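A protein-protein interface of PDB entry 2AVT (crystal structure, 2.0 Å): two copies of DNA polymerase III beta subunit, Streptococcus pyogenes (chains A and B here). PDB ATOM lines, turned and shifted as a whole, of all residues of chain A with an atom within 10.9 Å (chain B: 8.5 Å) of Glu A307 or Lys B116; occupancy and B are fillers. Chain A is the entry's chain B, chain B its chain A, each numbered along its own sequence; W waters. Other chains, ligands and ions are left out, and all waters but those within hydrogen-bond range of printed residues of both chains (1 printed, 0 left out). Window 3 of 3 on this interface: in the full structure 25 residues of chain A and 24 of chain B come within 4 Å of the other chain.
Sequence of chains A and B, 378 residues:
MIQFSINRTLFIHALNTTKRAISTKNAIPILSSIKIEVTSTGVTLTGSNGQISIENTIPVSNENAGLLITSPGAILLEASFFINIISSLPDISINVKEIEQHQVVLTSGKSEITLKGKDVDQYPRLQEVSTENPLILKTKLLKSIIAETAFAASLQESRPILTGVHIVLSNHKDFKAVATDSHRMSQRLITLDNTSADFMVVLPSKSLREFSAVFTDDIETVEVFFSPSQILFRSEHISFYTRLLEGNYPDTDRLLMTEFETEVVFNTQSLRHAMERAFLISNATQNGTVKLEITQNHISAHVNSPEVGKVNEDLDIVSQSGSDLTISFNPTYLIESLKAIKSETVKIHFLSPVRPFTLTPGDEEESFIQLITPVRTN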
ATOM      1  N   LEU A 280      -8.522  19.922  14.944  1.00  0.00           N
ATOM      2  CA  LEU A 280      -9.925  19.572  14.737  1.00  0.00           C
ATOM      3  C   LEU A 280     -10.824  20.762  15.018  1.00  0.00           C
ATOM      4  O   LEU A 280     -11.839  20.947  14.349  1.00  0.00           O
ATOM      5  CB  LEU A 280     -10.340  18.400  15.628  1.00  0.00           C
ATOM      6  CG  LEU A 280      -9.807  17.038  15.201  1.00  0.00           C
ATOM      7  CD1 LEU A 280     -10.253  15.985  16.198  1.00  0.00           C
ATOM      8  CD2 LEU A 280     -10.321  16.696  13.797  1.00  0.00           C
ATOM      9  N   ILE A 281     -10.462  21.571  16.007  1.00  0.00           N
ATOM     10  CA  ILE A 281     -11.261  22.745  16.345  1.00  0.00           C
ATOM     11  C   ILE A 281     -10.828  23.995  15.582  1.00  0.00           C
ATOM     12  O   ILE A 281     -11.669  24.747  15.104  1.00  0.00           O
ATOM     13  CB  ILE A 281     -11.213  23.043  17.861  1.00  0.00           C
ATOM     14  CG1 ILE A 281     -11.822  21.873  18.636  1.00  0.00           C
ATOM     15  CG2 ILE A 281     -11.937  24.353  18.162  1.00  0.00           C
ATOM     16  CD1 ILE A 281     -13.254  21.540  18.270  1.00  0.00           C
ATOM     17  N   ALA A 284     -11.887  24.791  11.935  1.00  0.00           N
ATOM     18  CA  ALA A 284     -13.272  25.208  11.761  1.00  0.00           C
ATOM     19  C   ALA A 284     -13.324  26.536  11.016  1.00  0.00           C
ATOM     20  O   ALA A 284     -14.274  26.813  10.294  1.00  0.00           O
ATOM     21  CB  ALA A 284     -13.952  25.348  13.118  1.00  0.00           C
ATOM     22  N   THR A 285     -12.298  27.356  11.199  1.00  0.00           N
ATOM     23  CA  THR A 285     -12.236  28.648  10.530  1.00  0.00           C
ATOM     24  C   THR A 285     -10.999  28.687   9.643  1.00  0.00           C
ATOM     25  O   THR A 285     -10.119  27.831   9.754  1.00  0.00           O
ATOM     26  CB  THR A 285     -12.150  29.798  11.544  1.00  0.00           C
ATOM     27  OG1 THR A 285     -10.830  29.848  12.095  1.00  0.00           O
ATOM     28  CG2 THR A 285     -13.152  29.587  12.677  1.00  0.00           C
ATOM     29  N   GLN A 286     -10.935  29.679   8.760  1.00  0.00           N
ATOM     30  CA  GLN A 286      -9.796  29.825   7.864  1.00  0.00           C
ATOM     31  C   GLN A 286      -8.713  30.559   8.657  1.00  0.00           C
ATOM     32  O   GLN A 286      -8.988  31.550   9.328  1.00  0.00           O
ATOM     33  CB  GLN A 286     -10.210  30.622   6.614  1.00  0.00           C
ATOM     34  CG  GLN A 286      -9.284  30.464   5.401  1.00  0.00           C
ATOM     35  CD  GLN A 286      -9.871  31.056   4.120  1.00  0.00           C
ATOM     36  OE1 GLN A 286     -10.203  32.244   4.062  1.00  0.00           O
ATOM     37  NE2 GLN A 286      -9.999  30.226   3.086  1.00  0.00           N
ATOM     38  N   VAL A 303      -7.589  26.810  21.910  1.00  0.00           N
ATOM     39  CA  VAL A 303      -8.198  27.089  20.615  1.00  0.00           C
ATOM     40  C   VAL A 303      -9.605  27.587  20.909  1.00  0.00           C
ATOM     41  O   VAL A 303     -10.279  27.068  21.806  1.00  0.00           O
ATOM     42  CB  VAL A 303      -8.326  25.829  19.734  1.00  0.00           C
ATOM     43  CG1 VAL A 303      -9.050  26.184  18.439  1.00  0.00           C
ATOM     44  CG2 VAL A 303      -6.947  25.259  19.424  1.00  0.00           C
ATOM     45  N   ASN A 304     -10.042  28.597  20.165  1.00  0.00           N
ATOM     46  CA  ASN A 304     -11.377  29.136  20.332  1.00  0.00           C
ATOM     47  C   ASN A 304     -12.004  29.404  18.966  1.00  0.00           C
ATOM     48  O   ASN A 304     -11.589  30.324  18.251  1.00  0.00           O
ATOM     49  CB  ASN A 304     -11.337  30.426  21.150  1.00  0.00           C
ATOM     50  CG  ASN A 304     -12.717  31.002  21.397  1.00  0.00           C
ATOM     51  OD1 ASN A 304     -12.863  31.996  22.109  1.00  0.00           O
ATOM     52  ND2 ASN A 304     -13.738  30.385  20.809  1.00  0.00           N
ATOM     53  N   SER A 305     -12.987  28.581  18.601  1.00  0.00           N
ATOM     54  CA  SER A 305     -13.690  28.740  17.330  1.00  0.00           C
ATOM     55  C   SER A 305     -15.135  29.096  17.627  1.00  0.00           C
ATOM     56  O   SER A 305     -15.974  28.219  17.840  1.00  0.00           O
ATOM     57  CB  SER A 305     -13.634  27.455  16.502  1.00  0.00           C
ATOM     58  OG  SER A 305     -12.397  27.330  15.818  1.00  0.00           O
ATOM     59  N   PRO A 306     -15.443  30.400  17.652  1.00  0.00           N
ATOM     60  CA  PRO A 306     -16.787  30.908  17.927  1.00  0.00           C
ATOM     61  C   PRO A 306     -17.893  30.144  17.208  1.00  0.00           C
ATOM     62  O   PRO A 306     -17.786  29.837  16.026  1.00  0.00           O
ATOM     63  CB  PRO A 306     -16.692  32.367  17.494  1.00  0.00           C
ATOM     64  CG  PRO A 306     -15.284  32.707  17.867  1.00  0.00           C
ATOM     65  CD  PRO A 306     -14.523  31.509  17.341  1.00  0.00           C
ATOM     66  N   GLU A 307     -18.941  29.822  17.953  1.00  0.00           N
ATOM     67  CA  GLU A 307     -20.098  29.095  17.443  1.00  0.00           C
ATOM     68  C   GLU A 307     -19.772  27.677  16.994  1.00  0.00           C
ATOM     69  O   GLU A 307     -20.630  26.995  16.448  1.00  0.00           O
ATOM     70  CB  GLU A 307     -20.769  29.877  16.302  1.00  0.00           C
ATOM     71  CG  GLU A 307     -20.218  29.616  14.902  1.00  0.00           C
ATOM     72  CD  GLU A 307     -20.677  30.652  13.881  1.00  0.00           C
ATOM     73  OE1 GLU A 307     -21.892  30.951  13.839  1.00  0.00           O
ATOM     74  OE2 GLU A 307     -19.828  31.165  13.118  1.00  0.00           O
ATOM     75  N   VAL A 308     -18.537  27.233  17.216  1.00  0.00           N
ATOM     76  CA  VAL A 308     -18.145  25.872  16.855  1.00  0.00           C
ATOM     77  C   VAL A 308     -17.633  25.128  18.096  1.00  0.00           C
ATOM     78  O   VAL A 308     -18.202  24.117  18.506  1.00  0.00           O
ATOM     79  CB  VAL A 308     -17.034  25.845  15.775  1.00  0.00           C
ATOM     80  CG1 VAL A 308     -16.704  24.393  15.419  1.00  0.00           C
ATOM     81  CG2 VAL A 308     -17.481  26.588  14.531  1.00  0.00           C
ATOM     82  N   GLY A 309     -16.557  25.629  18.696  1.00  0.00           N
ATOM     83  CA  GLY A 309     -16.024  24.975  19.873  1.00  0.00           C
ATOM     84  C   GLY A 309     -14.746  25.593  20.412  1.00  0.00           C
ATOM     85  O   GLY A 309     -14.264  26.602  19.901  1.00  0.00           O
ATOM     86  N   LYS A 310     -14.203  24.994  21.461  1.00  0.00           N
ATOM     87  CA  LYS A 310     -12.967  25.491  22.041  1.00  0.00           C
ATOM     88  C   LYS A 310     -12.177  24.336  22.647  1.00  0.00           C
ATOM     89  O   LYS A 310     -12.747  23.305  23.012  1.00  0.00           O
ATOM     90  CB  LYS A 310     -13.257  26.542  23.121  1.00  0.00           C
ATOM     91  CG  LYS A 310     -13.960  25.988  24.339  1.00  0.00           C
ATOM     92  CD  LYS A 310     -14.076  27.022  25.452  1.00  0.00           C
ATOM     93  CE  LYS A 310     -14.952  28.184  25.057  1.00  0.00           C
ATOM     94  NZ  LYS A 310     -15.299  29.006  26.250  1.00  0.00           N
ATOM     95  N   VAL A 311     -10.862  24.507  22.720  1.00  0.00           N
ATOM     96  CA  VAL A 311      -9.984  23.501  23.298  1.00  0.00           C
ATOM     97  C   VAL A 311      -9.103  24.149  24.371  1.00  0.00           C
ATOM     98  O   VAL A 311      -8.568  25.241  24.183  1.00  0.00           O
ATOM     99  CB  VAL A 311      -9.044  22.875  22.247  1.00  0.00           C
ATOM    100  CG1 VAL A 311      -8.182  21.806  22.904  1.00  0.00           C
ATOM    101  CG2 VAL A 311      -9.845  22.264  21.121  1.00  0.00           C
ATOM    102  N   ILE B  75     -29.289  16.127  23.188  1.00  0.00           N
ATOM    103  CA  ILE B  75     -28.605  17.144  22.404  1.00  0.00           C
ATOM    104  C   ILE B  75     -28.238  16.633  21.024  1.00  0.00           C
ATOM    105  O   ILE B  75     -28.144  15.422  20.814  1.00  0.00           O
ATOM    106  CB  ILE B  75     -27.309  17.625  23.130  1.00  0.00           C
ATOM    107  CG1 ILE B  75     -26.758  18.883  22.458  1.00  0.00           C
ATOM    108  CG2 ILE B  75     -26.233  16.539  23.094  1.00  0.00           C
ATOM    109  CD1 ILE B  75     -25.492  19.409  23.114  1.00  0.00           C
ATOM    110  N   LEU B  76     -28.055  17.567  20.089  1.00  0.00           N
ATOM    111  CA  LEU B  76     -27.654  17.275  18.718  1.00  0.00           C
ATOM    112  C   LEU B  76     -26.255  17.865  18.465  1.00  0.00           C
ATOM    113  O   LEU B  76     -25.982  19.012  18.821  1.00  0.00           O
ATOM    114  CB  LEU B  76     -28.631  17.905  17.715  1.00  0.00           C
ATOM    115  CG  LEU B  76     -30.133  17.602  17.788  1.00  0.00           C
ATOM    116  CD1 LEU B  76     -30.843  18.313  16.629  1.00  0.00           C
ATOM    117  CD2 LEU B  76     -30.358  16.096  17.702  1.00  0.00           C
ATOM    118  N   LEU B  77     -25.392  17.090  17.820  1.00  0.00           N
ATOM    119  CA  LEU B  77     -24.032  17.513  17.505  1.00  0.00           C
ATOM    120  C   LEU B  77     -23.730  17.055  16.081  1.00  0.00           C
ATOM    121  O   LEU B  77     -24.274  16.036  15.640  1.00  0.00           O
ATOM    122  CB  LEU B  77     -23.036  16.851  18.480  1.00  0.00           C
ATOM    123  CG  LEU B  77     -23.161  17.210  19.964  1.00  0.00           C
ATOM    124  CD1 LEU B  77     -22.334  16.253  20.835  1.00  0.00           C
ATOM    125  CD2 LEU B  77     -22.703  18.645  20.156  1.00  0.00           C
ATOM    126  N   GLU B  78     -22.897  17.796  15.349  1.00  0.00           N
ATOM    127  CA  GLU B  78     -22.555  17.376  13.987  1.00  0.00           C
ATOM    128  C   GLU B  78     -21.867  16.030  14.139  1.00  0.00           C
ATOM    129  O   GLU B  78     -20.843  15.923  14.811  1.00  0.00           O
ATOM    130  CB  GLU B  78     -21.602  18.370  13.317  1.00  0.00           C
ATOM    131  CG  GLU B  78     -22.241  19.685  12.918  1.00  0.00           C
ATOM    132  CD  GLU B  78     -23.364  19.504  11.916  1.00  0.00           C
ATOM    133  OE1 GLU B  78     -23.211  18.673  11.000  1.00  0.00           O
ATOM    134  OE2 GLU B  78     -24.389  20.202  12.036  1.00  0.00           O
ATOM    135  N   PHE B  81     -17.989  15.322  12.781  1.00  0.00           N
ATOM    136  CA  PHE B  81     -17.137  16.176  13.584  1.00  0.00           C
ATOM    137  C   PHE B  81     -17.043  15.656  15.033  1.00  0.00           C
ATOM    138  O   PHE B  81     -15.951  15.540  15.599  1.00  0.00           O
ATOM    139  CB  PHE B  81     -17.701  17.596  13.534  1.00  0.00           C
ATOM    140  CG  PHE B  81     -16.930  18.590  14.349  1.00  0.00           C
ATOM    141  CD1 PHE B  81     -15.599  18.848  14.079  1.00  0.00           C
ATOM    142  CD2 PHE B  81     -17.546  19.276  15.381  1.00  0.00           C
ATOM    143  CE1 PHE B  81     -14.894  19.775  14.827  1.00  0.00           C
ATOM    144  CE2 PHE B  81     -16.845  20.201  16.130  1.00  0.00           C
ATOM    145  CZ  PHE B  81     -15.516  20.448  15.848  1.00  0.00           C
ATOM    146  N   PHE B  82     -18.185  15.320  15.622  1.00  0.00           N
ATOM    147  CA  PHE B  82     -18.204  14.837  16.994  1.00  0.00           C
ATOM    148  C   PHE B  82     -17.406  13.558  17.155  1.00  0.00           C
ATOM    149  O   PHE B  82     -16.641  13.403  18.111  1.00  0.00           O
ATOM    150  CB  PHE B  82     -19.642  14.586  17.451  1.00  0.00           C
ATOM    151  CG  PHE B  82     -19.741  14.030  18.840  1.00  0.00           C
ATOM    152  CD1 PHE B  82     -19.236  14.740  19.919  1.00  0.00           C
ATOM    153  CD2 PHE B  82     -20.352  12.806  19.071  1.00  0.00           C
ATOM    154  CE1 PHE B  82     -19.347  14.239  21.212  1.00  0.00           C
ATOM    155  CE2 PHE B  82     -20.464  12.299  20.358  1.00  0.00           C
ATOM    156  CZ  PHE B  82     -19.962  13.019  21.430  1.00  0.00           C
ATOM    157  N   ILE B  85     -13.685  14.057  17.030  1.00  0.00           N
ATOM    158  CA  ILE B  85     -13.222  14.609  18.303  1.00  0.00           C
ATOM    159  C   ILE B  85     -13.083  13.502  19.361  1.00  0.00           C
ATOM    160  O   ILE B  85     -12.022  13.355  19.981  1.00  0.00           O
ATOM    161  CB  ILE B  85     -14.170  15.701  18.802  1.00  0.00           C
ATOM    162  CG1 ILE B  85     -13.905  16.985  18.015  1.00  0.00           C
ATOM    163  CG2 ILE B  85     -13.957  15.956  20.293  1.00  0.00           C
ATOM    164  CD1 ILE B  85     -15.056  17.919  18.008  1.00  0.00           C
ATOM    165  N   ILE B  99     -23.577  22.083  29.265  1.00  0.00           N
ATOM    166  CA  ILE B  99     -23.660  23.341  29.991  1.00  0.00           C
ATOM    167  C   ILE B  99     -24.659  24.195  29.232  1.00  0.00           C
ATOM    168  O   ILE B  99     -25.314  23.703  28.312  1.00  0.00           O
ATOM    169  CB  ILE B  99     -22.292  24.059  30.081  1.00  0.00           C
ATOM    170  CG1 ILE B  99     -21.728  24.322  28.683  1.00  0.00           C
ATOM    171  CG2 ILE B  99     -21.317  23.202  30.878  1.00  0.00           C
ATOM    172  CD1 ILE B  99     -20.421  25.122  28.694  1.00  0.00           C
ATOM    173  N   GLU B 100     -24.776  25.465  29.604  1.00  0.00           N
ATOM    174  CA  GLU B 100     -25.728  26.365  28.973  1.00  0.00           C
ATOM    175  C   GLU B 100     -25.571  26.539  27.474  1.00  0.00           C
ATOM    176  O   GLU B 100     -24.480  26.399  26.926  1.00  0.00           O
ATOM    177  CB  GLU B 100     -25.660  27.749  29.628  1.00  0.00           C
ATOM    178  CG  GLU B 100     -24.294  28.415  29.521  1.00  0.00           C
ATOM    179  CD  GLU B 100     -24.313  29.858  29.997  1.00  0.00           C
ATOM    180  OE1 GLU B 100     -24.677  30.097  31.172  1.00  0.00           O
ATOM    181  OE2 GLU B 100     -23.966  30.752  29.190  1.00  0.00           O
ATOM    182  N   GLN B 101     -26.687  26.858  26.826  1.00  0.00           N
ATOM    183  CA  GLN B 101     -26.738  27.103  25.391  1.00  0.00           C
ATOM    184  C   GLN B 101     -26.357  25.908  24.522  1.00  0.00           C
ATOM    185  O   GLN B 101     -25.667  26.061  23.518  1.00  0.00           O
ATOM    186  CB  GLN B 101     -25.846  28.301  25.057  1.00  0.00           C
ATOM    187  CG  GLN B 101     -26.148  29.523  25.910  1.00  0.00           C
ATOM    188  CD  GLN B 101     -25.144  30.642  25.714  1.00  0.00           C
ATOM    189  OE1 GLN B 101     -23.931  30.419  25.757  1.00  0.00           O
ATOM    190  NE2 GLN B 101     -25.642  31.856  25.507  1.00  0.00           N
ATOM    191  N   HIS B 102     -26.817  24.726  24.919  1.00  0.00           N
ATOM    192  CA  HIS B 102     -26.572  23.484  24.194  1.00  0.00           C
ATOM    193  C   HIS B 102     -25.118  23.232  23.823  1.00  0.00           C
ATOM    194  O   HIS B 102     -24.790  22.955  22.668  1.00  0.00           O
ATOM    195  CB  HIS B 102     -27.464  23.427  22.946  1.00  0.00           C
ATOM    196  CG  HIS B 102     -28.921  23.591  23.255  1.00  0.00           C
ATOM    197  ND1 HIS B 102     -29.553  24.817  23.237  1.00  0.00           N
ATOM    198  CD2 HIS B 102     -29.845  22.699  23.683  1.00  0.00           C
ATOM    199  CE1 HIS B 102     -30.802  24.674  23.644  1.00  0.00           C
ATOM    200  NE2 HIS B 102     -31.004  23.399  23.920  1.00  0.00           N
ATOM    201  N   GLN B 103     -24.253  23.314  24.826  1.00  0.00           N
ATOM    202  CA  GLN B 103     -22.828  23.075  24.649  1.00  0.00           C
ATOM    203  C   GLN B 103     -22.473  21.885  25.512  1.00  0.00           C
ATOM    204  O   GLN B 103     -23.081  21.682  26.561  1.00  0.00           O
ATOM    205  CB  GLN B 103     -22.015  24.281  25.137  1.00  0.00           C
ATOM    206  CG  GLN B 103     -22.282  25.585  24.412  1.00  0.00           C
ATOM    207  CD  GLN B 103     -21.445  26.727  24.973  1.00  0.00           C
ATOM    208  OE1 GLN B 103     -21.822  27.367  25.963  1.00  0.00           O
ATOM    209  NE2 GLN B 103     -20.293  26.975  24.352  1.00  0.00           N
ATOM    210  N   VAL B 104     -21.515  21.079  25.071  1.00  0.00           N
ATOM    211  CA  VAL B 104     -21.078  19.952  25.879  1.00  0.00           C
ATOM    212  C   VAL B 104     -19.582  20.053  26.088  1.00  0.00           C
ATOM    213  O   VAL B 104     -18.824  20.330  25.155  1.00  0.00           O
ATOM    214  CB  VAL B 104     -21.387  18.573  25.236  1.00  0.00           C
ATOM    215  CG1 VAL B 104     -22.890  18.313  25.268  1.00  0.00           C
ATOM    216  CG2 VAL B 104     -20.867  18.523  23.819  1.00  0.00           C
ATOM    217  N   VAL B 105     -19.166  19.835  27.327  1.00  0.00           N
ATOM    218  CA  VAL B 105     -17.762  19.871  27.681  1.00  0.00           C
ATOM    219  C   VAL B 105     -17.319  18.423  27.757  1.00  0.00           C
ATOM    220  O   VAL B 105     -17.855  17.641  28.553  1.00  0.00           O
ATOM    221  CB  VAL B 105     -17.555  20.528  29.053  1.00  0.00           C
ATOM    222  CG1 VAL B 105     -16.073  20.534  29.413  1.00  0.00           C
ATOM    223  CG2 VAL B 105     -18.138  21.934  29.046  1.00  0.00           C
ATOM    224  N   LEU B 106     -16.348  18.073  26.920  1.00  0.00           N
ATOM    225  CA  LEU B 106     -15.809  16.730  26.867  1.00  0.00           C
ATOM    226  C   LEU B 106     -14.451  16.770  27.574  1.00  0.00           C
ATOM    227  O   LEU B 106     -13.564  17.536  27.175  1.00  0.00           O
ATOM    228  CB  LEU B 106     -15.617  16.304  25.412  1.00  0.00           C
ATOM    229  CG  LEU B 106     -16.820  16.434  24.463  1.00  0.00           C
ATOM    230  CD1 LEU B 106     -16.386  16.109  23.039  1.00  0.00           C
ATOM    231  CD2 LEU B 106     -17.938  15.474  24.904  1.00  0.00           C
ATOM    232  N   ILE B 113     -12.397  19.734  25.750  1.00  0.00           N
ATOM    233  CA  ILE B 113     -12.930  20.240  24.484  1.00  0.00           C
ATOM    234  C   ILE B 113     -14.418  20.545  24.610  1.00  0.00           C
ATOM    235  O   ILE B 113     -15.219  19.670  24.954  1.00  0.00           O
ATOM    236  CB  ILE B 113     -12.717  19.204  23.343  1.00  0.00           C
ATOM    237  CG1 ILE B 113     -11.218  19.013  23.099  1.00  0.00           C
ATOM    238  CG2 ILE B 113     -13.418  19.675  22.055  1.00  0.00           C
ATOM    239  CD1 ILE B 113     -10.871  17.824  22.218  1.00  0.00           C
ATOM    240  N   THR B 114     -14.787  21.792  24.351  1.00  0.00           N
ATOM    241  CA  THR B 114     -16.186  22.188  24.431  1.00  0.00           C
ATOM    242  C   THR B 114     -16.747  22.335  23.024  1.00  0.00           C
ATOM    243  O   THR B 114     -16.128  22.969  22.167  1.00  0.00           O
ATOM    244  CB  THR B 114     -16.334  23.515  25.185  1.00  0.00           C
ATOM    245  OG1 THR B 114     -15.673  23.404  26.450  1.00  0.00           O
ATOM    246  CG2 THR B 114     -17.812  23.857  25.407  1.00  0.00           C
ATOM    247  N   LEU B 115     -17.914  21.738  22.786  1.00  0.00           N
ATOM    248  CA  LEU B 115     -18.560  21.797  21.475  1.00  0.00           C
ATOM    249  C   LEU B 115     -19.942  22.433  21.542  1.00  0.00           C
ATOM    250  O   LEU B 115     -20.676  22.245  22.515  1.00  0.00           O
ATOM    251  CB  LEU B 115     -18.710  20.395  20.891  1.00  0.00           C
ATOM    252  CG  LEU B 115     -17.435  19.567  20.808  1.00  0.00           C
ATOM    253  CD1 LEU B 115     -17.781  18.168  20.345  1.00  0.00           C
ATOM    254  CD2 LEU B 115     -16.432  20.250  19.868  1.00  0.00           C
ATOM    255  N   LYS B 116     -20.297  23.186  20.504  1.00  0.00           N
ATOM    256  CA  LYS B 116     -21.615  23.807  20.457  1.00  0.00           C
ATOM    257  C   LYS B 116     -22.560  22.832  19.766  1.00  0.00           C
ATOM    258  O   LYS B 116     -22.221  22.248  18.729  1.00  0.00           O
ATOM    259  CB  LYS B 116     -21.562  25.142  19.695  1.00  0.00           C
ATOM    260  CG  LYS B 116     -22.922  25.805  19.453  1.00  0.00           C
ATOM    261  CD  LYS B 116     -23.766  25.872  20.725  1.00  0.00           C
ATOM    262  CE  LYS B 116     -24.359  27.258  20.931  1.00  0.00           C
ATOM    263  NZ  LYS B 116     -25.065  27.747  19.715  1.00  0.00           N
ATOM    264  N   GLY B 117     -23.735  22.639  20.354  1.00  0.00           N
ATOM    265  CA  GLY B 117     -24.708  21.732  19.766  1.00  0.00           C
ATOM    266  C   GLY B 117     -26.068  22.383  19.569  1.00  0.00           C
ATOM    267  O   GLY B 117     -26.210  23.597  19.670  1.00  0.00           O
ATOM    268  N   LYS B 118     -27.082  21.578  19.290  1.00  0.00           N
ATOM    269  CA  LYS B 118     -28.416  22.124  19.080  1.00  0.00           C
ATOM    270  C   LYS B 118     -29.454  21.370  19.879  1.00  0.00           C
ATOM    271  O   LYS B 118     -29.252  20.208  20.242  1.00  0.00           O
ATOM    272  CB  LYS B 118     -28.796  22.059  17.600  1.00  0.00           C
ATOM    273  CG  LYS B 118     -27.928  22.893  16.670  1.00  0.00           C
ATOM    274  CD  LYS B 118     -28.509  22.879  15.264  1.00  0.00           C
ATOM    275  CE  LYS B 118     -27.669  23.692  14.285  1.00  0.00           C
ATOM    276  NZ  LYS B 118     -26.370  23.035  14.003  1.00  0.00           N
ATOM    277  N   ASP B 119     -30.567  22.047  20.143  1.00  0.00           N
ATOM    278  CA  ASP B 119     -31.685  21.474  20.880  1.00  0.00           C
ATOM    279  C   ASP B 119     -32.271  20.344  20.033  1.00  0.00           C
ATOM    280  O   ASP B 119     -32.433  20.493  18.824  1.00  0.00           O
ATOM    281  CB  ASP B 119     -32.751  22.545  21.110  1.00  0.00           C
ATOM    282  CG  ASP B 119     -33.796  22.120  22.110  1.00  0.00           C
ATOM    283  OD1 ASP B 119     -34.515  21.124  21.859  1.00  0.00           O
ATOM    284  OD2 ASP B 119     -33.887  22.785  23.160  1.00  0.00           O
ATOM    285  N   GLN B 122     -35.124  20.205  17.171  1.00  0.00           N
ATOM    286  CA  GLN B 122     -34.881  20.545  15.772  1.00  0.00           C
ATOM    287  C   GLN B 122     -34.815  19.283  14.908  1.00  0.00           C
ATOM    288  O   GLN B 122     -34.882  19.354  13.680  1.00  0.00           O
ATOM    289  CB  GLN B 122     -33.577  21.343  15.633  1.00  0.00           C
ATOM    290  CG  GLN B 122     -33.610  22.687  16.352  1.00  0.00           C
ATOM    291  CD  GLN B 122     -32.402  23.558  16.055  1.00  0.00           C
ATOM    292  OE1 GLN B 122     -31.931  23.621  14.920  1.00  0.00           O
ATOM    293  NE2 GLN B 122     -31.910  24.257  17.073  1.00  0.00           N
HETATM  294  O   HOH W   1     -12.877  23.625  26.418  1.00  0.00           O
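Among the printed residues, merely in contact across the chains: Gly A309 with Thr B114 (3.0 Å), Leu A280 with Phe B81 (3.3 Å), Lys A310 with Ile B113 (3.4 Å), Ile A281 with Phe B81 (3.5 Å), Ile A281 with Leu B115 (3.8 Å), Val A308 with Leu B115 (3.8 Å), Glu A307 with Lys B116 (3.9 Å) and Leu A280 with Ile B85 (3.9 Å).
Of chain B, only Lys B116 (3.9 Å) comes within 4 Å of Glu A307.
Of the printed residues of chain B, Val A308 touches Leu B115 (3.8 Å) and Lys B116 (3.0 Å).
Printed residues of chain B within 4 Å of Gly A309: Thr B114 (3.0 Å).
No residue of chain A comes within 4 Å of Gln B101.
Printed residues of chain A within 4 Å of Ile B113: Lys A310 (3.4 Å).
Of chain A, only Ile A281 and Val A308 come within 4 Å of Leu B115.
Lys B116 touches just these residues of chain A: Glu A307 and Val A308.
No residue of chain A comes within 4 Å of Gly B117.
The nearest residue of chain B that does not touch Glu A307 is Gly B117 (6.6 Å).
The nearest residue of chain A that does not touch Lys B116 is Gly A309 (4.7 Å).
No position is printed for both chains.
Of the 10 pairs that touch across the chains among the printed residues, none has its exchanged pair printed and touching as well.
Hydrophobic or aromatic side chains of chain A within 4 Å of the printed part of chain B: Leu A280 and Ile A281.
Of the 23 printed residues of chain B, 6 touch a printed residue of chain A.
Printed residues of chain B that touch a printed residue of chain A: Phe B81, Ile B85, Ile B113, Thr B114, Leu B115 and Lys B116.
Among the printed residues, 10 pairs touch across the chains.
N of Leu B115 lies within hydrogen-bond range of O of Val B104.
O of Ile B113 sits at hydrogen-bond distance from N of Leu B106 (2.8 Å).
The side-chain hydroxyl of Ser A305 is in hydrogen-bond range of the backbone carbonyl oxygen of Ile A281, at 2.8 Å.
Water W1 lies within hydrogen-bond range of the side-chain hydroxyl of Thr B114 (2.8 Å) and the backbone carbonyl oxygen of Lys A310 (3.4 Å).
The backbone carbonyl oxygen of Lys A310 sits at hydrogen-bond distance from the backbone NH of Thr B114 (2.9 Å).
The backbone NH of Lys B116 lies within hydrogen-bond range of the backbone carbonyl oxygen of Val A308 (3.0 Å).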
